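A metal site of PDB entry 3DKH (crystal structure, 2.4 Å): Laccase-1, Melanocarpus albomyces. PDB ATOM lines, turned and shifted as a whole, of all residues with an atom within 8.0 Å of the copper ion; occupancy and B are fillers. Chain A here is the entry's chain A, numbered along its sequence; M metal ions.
The backbone carbonyl oxygen (O) of Leu 513 sits at hydrogen-bond distance from the backbone NH (N) of Cys 503 (3.2 Å). O of His 508 is in hydrogen-bond range of N of Leu 513, 3.0 Å away. O of His 431 sits at hydrogen-bond distance from N of Leu 481, 2.7 Å away. The backbone carbonyl oxygen (O) of Leu 429 is in hydrogen-bond range of a ring nitrogen (NE2) of His 431. SG of Cys 503 sits close to N of Ile 505 (3.5 Å).
Residues that only touch the copper ion: Ile 505 (3.8 Å) and Leu 513 (3.7 Å). The nearest printed residue that does not touch the copper ion is Pro 430 (4.3 Å).
The copper ion is bound by a ring nitrogen (ND1) of His 431. The copper ion is bound by the side-chain sulfur (SG) of Cys 503 (2.2 Å). The copper ion is bound by ND1 of His 508.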
ATOM      1  N   GLU A 235     -33.343  19.503  -3.522  1.00  0.00           N
ATOM      2  CA  GLU A 235     -32.365  20.192  -4.383  1.00  0.00           C
ATOM      3  C   GLU A 235     -32.948  21.427  -5.045  1.00  0.00           C
ATOM      4  O   GLU A 235     -32.299  22.465  -5.079  1.00  0.00           O
ATOM      5  CB  GLU A 235     -31.799  19.252  -5.463  1.00  0.00           C
ATOM      6  CG  GLU A 235     -30.578  19.777  -6.257  1.00  0.00           C
ATOM      7  CD  GLU A 235     -30.911  20.584  -7.522  1.00  0.00           C
ATOM      8  OE1 GLU A 235     -32.016  20.410  -8.075  1.00  0.00           O
ATOM      9  OE2 GLU A 235     -30.072  21.399  -7.941  1.00  0.00           O
ATOM     10  N   HIS A 237     -34.590  24.840  -6.157  1.00  0.00           N
ATOM     11  CA  HIS A 237     -34.732  26.190  -5.617  1.00  0.00           C
ATOM     12  C   HIS A 237     -35.751  26.882  -6.529  1.00  0.00           C
ATOM     13  O   HIS A 237     -35.572  26.953  -7.756  1.00  0.00           O
ATOM     14  CB  HIS A 237     -33.437  26.953  -5.659  1.00  0.00           C
ATOM     15  CG  HIS A 237     -32.337  26.336  -4.866  1.00  0.00           C
ATOM     16  ND1 HIS A 237     -31.798  25.106  -5.171  1.00  0.00           N
ATOM     17  CD2 HIS A 237     -31.626  26.801  -3.816  1.00  0.00           C
ATOM     18  CE1 HIS A 237     -30.799  24.853  -4.348  1.00  0.00           C
ATOM     19  NE2 HIS A 237     -30.677  25.870  -3.516  1.00  0.00           N
ATOM     20  N   VAL A 361     -15.275  26.222   0.963  1.00  0.00           N
ATOM     21  CA  VAL A 361     -16.036  25.116   0.396  1.00  0.00           C
ATOM     22  C   VAL A 361     -15.290  24.704  -0.872  1.00  0.00           C
ATOM     23  O   VAL A 361     -14.990  25.541  -1.719  1.00  0.00           O
ATOM     24  CB  VAL A 361     -17.488  25.549   0.037  1.00  0.00           C
ATOM     25  CG1 VAL A 361     -18.246  24.419  -0.636  1.00  0.00           C
ATOM     26  CG2 VAL A 361     -18.216  25.993   1.280  1.00  0.00           C
ATOM     27  N   TRP A 373     -17.891  16.769  -1.323  1.00  0.00           N
ATOM     28  CA  TRP A 373     -17.868  18.179  -0.916  1.00  0.00           C
ATOM     29  C   TRP A 373     -17.104  18.410   0.390  1.00  0.00           C
ATOM     30  O   TRP A 373     -17.450  17.851   1.418  1.00  0.00           O
ATOM     31  CB  TRP A 373     -19.296  18.709  -0.809  1.00  0.00           C
ATOM     32  CG  TRP A 373     -19.979  18.807  -2.130  1.00  0.00           C
ATOM     33  CD1 TRP A 373     -20.796  17.872  -2.690  1.00  0.00           C
ATOM     34  CD2 TRP A 373     -19.868  19.867  -3.077  1.00  0.00           C
ATOM     35  NE1 TRP A 373     -21.197  18.280  -3.937  1.00  0.00           N
ATOM     36  CE2 TRP A 373     -20.644  19.502  -4.210  1.00  0.00           C
ATOM     37  CE3 TRP A 373     -19.180  21.106  -3.091  1.00  0.00           C
ATOM     38  CZ2 TRP A 373     -20.756  20.330  -5.356  1.00  0.00           C
ATOM     39  CZ3 TRP A 373     -19.291  21.934  -4.238  1.00  0.00           C
ATOM     40  CH2 TRP A 373     -20.075  21.533  -5.353  1.00  0.00           C
ATOM     41  N   ASN A 421     -16.853  30.049  -1.712  1.00  0.00           N
ATOM     42  CA  ASN A 421     -17.397  29.056  -2.656  1.00  0.00           C
ATOM     43  C   ASN A 421     -16.475  28.592  -3.791  1.00  0.00           C
ATOM     44  O   ASN A 421     -16.711  28.931  -4.952  1.00  0.00           O
ATOM     45  CB  ASN A 421     -18.696  29.586  -3.267  1.00  0.00           C
ATOM     46  CG  ASN A 421     -19.618  28.478  -3.741  1.00  0.00           C
ATOM     47  OD1 ASN A 421     -19.264  27.296  -3.759  1.00  0.00           O
ATOM     48  ND2 ASN A 421     -20.835  28.857  -4.116  1.00  0.00           N
ATOM     49  N   LEU A 429     -21.029  25.845  -7.938  1.00  0.00           N
ATOM     50  CA  LEU A 429     -22.486  25.823  -7.889  1.00  0.00           C
ATOM     51  C   LEU A 429     -22.997  26.612  -6.688  1.00  0.00           C
ATOM     52  O   LEU A 429     -22.275  26.755  -5.696  1.00  0.00           O
ATOM     53  CB  LEU A 429     -22.958  24.358  -7.785  1.00  0.00           C
ATOM     54  CG  LEU A 429     -22.870  23.452  -9.018  1.00  0.00           C
ATOM     55  CD1 LEU A 429     -23.074  22.000  -8.600  1.00  0.00           C
ATOM     56  CD2 LEU A 429     -23.914  23.848 -10.052  1.00  0.00           C
ATOM     57  N   PRO A 430     -24.231  27.185  -6.767  1.00  0.00           N
ATOM     58  CA  PRO A 430     -24.807  27.952  -5.653  1.00  0.00           C
ATOM     59  C   PRO A 430     -25.178  27.020  -4.484  1.00  0.00           C
ATOM     60  O   PRO A 430     -25.604  25.876  -4.705  1.00  0.00           O
ATOM     61  CB  PRO A 430     -26.064  28.568  -6.278  1.00  0.00           C
ATOM     62  CG  PRO A 430     -25.736  28.667  -7.707  1.00  0.00           C
ATOM     63  CD  PRO A 430     -25.081  27.337  -7.964  1.00  0.00           C
ATOM     64  N   HIS A 431     -24.973  27.489  -3.248  1.00  0.00           N
ATOM     65  CA  HIS A 431     -25.255  26.666  -2.067  1.00  0.00           C
ATOM     66  C   HIS A 431     -26.158  27.310  -1.016  1.00  0.00           C
ATOM     67  O   HIS A 431     -25.805  28.344  -0.463  1.00  0.00           O
ATOM     68  CB  HIS A 431     -23.949  26.218  -1.367  1.00  0.00           C
ATOM     69  CG  HIS A 431     -23.039  25.373  -2.221  1.00  0.00           C
ATOM     70  ND1 HIS A 431     -23.472  24.264  -2.899  1.00  0.00           N
ATOM     71  CD2 HIS A 431     -21.720  25.494  -2.495  1.00  0.00           C
ATOM     72  CE1 HIS A 431     -22.459  23.730  -3.560  1.00  0.00           C
ATOM     73  NE2 HIS A 431     -21.382  24.457  -3.329  1.00  0.00           N
ATOM     74  N   PRO A 432     -27.346  26.724  -0.742  1.00  0.00           N
ATOM     75  CA  PRO A 432     -28.260  27.250   0.271  1.00  0.00           C
ATOM     76  C   PRO A 432     -27.738  26.896   1.667  1.00  0.00           C
ATOM     77  O   PRO A 432     -27.941  25.792   2.158  1.00  0.00           O
ATOM     78  CB  PRO A 432     -29.577  26.550  -0.074  1.00  0.00           C
ATOM     79  CG  PRO A 432     -29.131  25.239  -0.635  1.00  0.00           C
ATOM     80  CD  PRO A 432     -28.000  25.652  -1.525  1.00  0.00           C
ATOM     81  N   MET A 433     -26.954  27.790   2.236  1.00  0.00           N
ATOM     82  CA  MET A 433     -26.378  27.566   3.559  1.00  0.00           C
ATOM     83  C   MET A 433     -27.382  27.743   4.690  1.00  0.00           C
ATOM     84  O   MET A 433     -28.086  28.743   4.783  1.00  0.00           O
ATOM     85  CB  MET A 433     -25.144  28.441   3.764  1.00  0.00           C
ATOM     86  CG  MET A 433     -24.005  28.120   2.802  1.00  0.00           C
ATOM     87  SD  MET A 433     -23.574  26.374   2.647  1.00  0.00           S
ATOM     88  CE  MET A 433     -22.455  26.158   3.977  1.00  0.00           C
ATOM     89  N   MET A 480     -28.347  32.047   0.525  1.00  0.00           N
ATOM     90  CA  MET A 480     -27.505  31.563  -0.564  1.00  0.00           C
ATOM     91  C   MET A 480     -26.038  31.941  -0.547  1.00  0.00           C
ATOM     92  O   MET A 480     -25.680  33.101  -0.360  1.00  0.00           O
ATOM     93  CB  MET A 480     -28.074  31.974  -1.922  1.00  0.00           C
ATOM     94  CG  MET A 480     -29.407  31.351  -2.280  1.00  0.00           C
ATOM     95  SD  MET A 480     -29.405  29.573  -2.171  1.00  0.00           S
ATOM     96  CE  MET A 480     -28.519  29.143  -3.635  1.00  0.00           C
ATOM     97  N   LEU A 481     -25.189  30.934  -0.750  1.00  0.00           N
ATOM     98  CA  LEU A 481     -23.758  31.143  -0.887  1.00  0.00           C
ATOM     99  C   LEU A 481     -23.670  31.153  -2.412  1.00  0.00           C
ATOM    100  O   LEU A 481     -23.944  30.144  -3.074  1.00  0.00           O
ATOM    101  CB  LEU A 481     -22.953  29.995  -0.274  1.00  0.00           C
ATOM    102  CG  LEU A 481     -21.468  29.798  -0.595  1.00  0.00           C
ATOM    103  CD1 LEU A 481     -20.601  30.933  -0.128  1.00  0.00           C
ATOM    104  CD2 LEU A 481     -20.988  28.493  -0.012  1.00  0.00           C
ATOM    105  N   HIS A 502     -24.689  23.570   7.336  1.00  0.00           N
ATOM    106  CA  HIS A 502     -24.552  22.851   6.103  1.00  0.00           C
ATOM    107  C   HIS A 502     -25.353  23.379   4.934  1.00  0.00           C
ATOM    108  O   HIS A 502     -26.262  24.202   5.100  1.00  0.00           O
ATOM    109  CB  HIS A 502     -24.947  21.375   6.339  1.00  0.00           C
ATOM    110  CG  HIS A 502     -26.402  21.159   6.616  1.00  0.00           C
ATOM    111  ND1 HIS A 502     -27.288  20.752   5.645  1.00  0.00           N
ATOM    112  CD2 HIS A 502     -27.123  21.306   7.758  1.00  0.00           C
ATOM    113  CE1 HIS A 502     -28.499  20.644   6.168  1.00  0.00           C
ATOM    114  NE2 HIS A 502     -28.422  20.977   7.451  1.00  0.00           N
ATOM    115  N   CYS A 503     -25.041  22.822   3.767  1.00  0.00           N
ATOM    116  CA  CYS A 503     -25.750  23.134   2.538  1.00  0.00           C
ATOM    117  C   CYS A 503     -26.992  22.268   2.659  1.00  0.00           C
ATOM    118  O   CYS A 503     -26.910  21.096   3.066  1.00  0.00           O
ATOM    119  CB  CYS A 503     -24.953  22.688   1.318  1.00  0.00           C
ATOM    120  SG  CYS A 503     -25.894  22.915  -0.182  1.00  0.00           S
ATOM    121  N   HIS A 504     -28.149  22.853   2.331  1.00  0.00           N
ATOM    122  CA  HIS A 504     -29.390  22.116   2.424  1.00  0.00           C
ATOM    123  C   HIS A 504     -29.798  21.274   1.203  1.00  0.00           C
ATOM    124  O   HIS A 504     -30.845  20.625   1.216  1.00  0.00           O
ATOM    125  CB  HIS A 504     -30.510  23.000   2.943  1.00  0.00           C
ATOM    126  CG  HIS A 504     -31.484  22.269   3.815  1.00  0.00           C
ATOM    127  ND1 HIS A 504     -32.287  21.253   3.341  1.00  0.00           N
ATOM    128  CD2 HIS A 504     -31.751  22.379   5.133  1.00  0.00           C
ATOM    129  CE1 HIS A 504     -33.012  20.770   4.327  1.00  0.00           C
ATOM    130  NE2 HIS A 504     -32.705  21.439   5.424  1.00  0.00           N
ATOM    131  N   ILE A 505     -28.976  21.298   0.142  1.00  0.00           N
ATOM    132  CA  ILE A 505     -29.216  20.429  -1.022  1.00  0.00           C
ATOM    133  C   ILE A 505     -28.810  19.061  -0.435  1.00  0.00           C
ATOM    134  O   ILE A 505     -27.682  18.906   0.053  1.00  0.00           O
ATOM    135  CB  ILE A 505     -28.321  20.777  -2.249  1.00  0.00           C
ATOM    136  CG1 ILE A 505     -28.863  22.010  -2.961  1.00  0.00           C
ATOM    137  CG2 ILE A 505     -28.241  19.582  -3.239  1.00  0.00           C
ATOM    138  CD1 ILE A 505     -27.909  22.654  -3.969  1.00  0.00           C
ATOM    139  N   ALA A 506     -29.785  18.154  -0.362  1.00  0.00           N
ATOM    140  CA  ALA A 506     -29.621  16.814   0.206  1.00  0.00           C
ATOM    141  C   ALA A 506     -28.403  16.063  -0.275  1.00  0.00           C
ATOM    142  O   ALA A 506     -27.642  15.532   0.532  1.00  0.00           O
ATOM    143  CB  ALA A 506     -30.850  15.990  -0.017  1.00  0.00           C
ATOM    144  N   TRP A 507     -28.169  16.142  -1.577  1.00  0.00           N
ATOM    145  CA  TRP A 507     -27.043  15.470  -2.226  1.00  0.00           C
ATOM    146  C   TRP A 507     -25.687  16.042  -1.818  1.00  0.00           C
ATOM    147  O   TRP A 507     -24.704  15.299  -1.671  1.00  0.00           O
ATOM    148  CB  TRP A 507     -27.191  15.512  -3.745  1.00  0.00           C
ATOM    149  CG  TRP A 507     -28.620  15.546  -4.330  1.00  0.00           C
ATOM    150  CD1 TRP A 507     -29.037  16.369  -5.338  1.00  0.00           C
ATOM    151  CD2 TRP A 507     -29.782  14.760  -3.958  1.00  0.00           C
ATOM    152  NE1 TRP A 507     -30.356  16.158  -5.627  1.00  0.00           N
ATOM    153  CE2 TRP A 507     -30.853  15.186  -4.799  1.00  0.00           C
ATOM    154  CE3 TRP A 507     -30.019  13.743  -2.999  1.00  0.00           C
ATOM    155  CZ2 TRP A 507     -32.153  14.633  -4.700  1.00  0.00           C
ATOM    156  CZ3 TRP A 507     -31.314  13.198  -2.899  1.00  0.00           C
ATOM    157  CH2 TRP A 507     -32.375  13.647  -3.757  1.00  0.00           C
ATOM    158  N   HIS A 508     -25.648  17.349  -1.577  1.00  0.00           N
ATOM    159  CA  HIS A 508     -24.423  18.035  -1.180  1.00  0.00           C
ATOM    160  C   HIS A 508     -24.004  17.808   0.269  1.00  0.00           C
ATOM    161  O   HIS A 508     -22.805  17.602   0.537  1.00  0.00           O
ATOM    162  CB  HIS A 508     -24.490  19.527  -1.542  1.00  0.00           C
ATOM    163  CG  HIS A 508     -24.564  19.791  -3.019  1.00  0.00           C
ATOM    164  ND1 HIS A 508     -24.783  21.043  -3.535  1.00  0.00           N
ATOM    165  CD2 HIS A 508     -24.450  18.958  -4.082  1.00  0.00           C
ATOM    166  CE1 HIS A 508     -24.805  20.976  -4.855  1.00  0.00           C
ATOM    167  NE2 HIS A 508     -24.601  19.723  -5.212  1.00  0.00           N
ATOM    168  N   VAL A 509     -24.964  17.778   1.186  1.00  0.00           N
ATOM    169  CA  VAL A 509     -24.681  17.513   2.608  1.00  0.00           C
ATOM    170  C   VAL A 509     -24.274  16.037   2.749  1.00  0.00           C
ATOM    171  O   VAL A 509     -23.461  15.688   3.610  1.00  0.00           O
ATOM    172  CB  VAL A 509     -25.861  17.933   3.569  1.00  0.00           C
ATOM    173  CG1 VAL A 509     -27.127  17.145   3.303  1.00  0.00           C
ATOM    174  CG2 VAL A 509     -25.433  17.810   5.024  1.00  0.00           C
ATOM    175  N   LEU A 513     -20.743  18.483   2.528  1.00  0.00           N
ATOM    176  CA  LEU A 513     -20.829  19.925   2.750  1.00  0.00           C
ATOM    177  C   LEU A 513     -21.493  20.296   4.067  1.00  0.00           C
ATOM    178  O   LEU A 513     -22.686  20.643   4.101  1.00  0.00           O
ATOM    179  CB  LEU A 513     -21.528  20.629   1.589  1.00  0.00           C
ATOM    180  CG  LEU A 513     -20.850  21.900   1.043  1.00  0.00           C
ATOM    181  CD1 LEU A 513     -21.358  22.134  -0.351  1.00  0.00           C
ATOM    182  CD2 LEU A 513     -21.094  23.121   1.925  1.00  0.00           C
HETATM  183 CU    CU M   1     -24.653  22.702  -1.973  1.00  0.00          CU
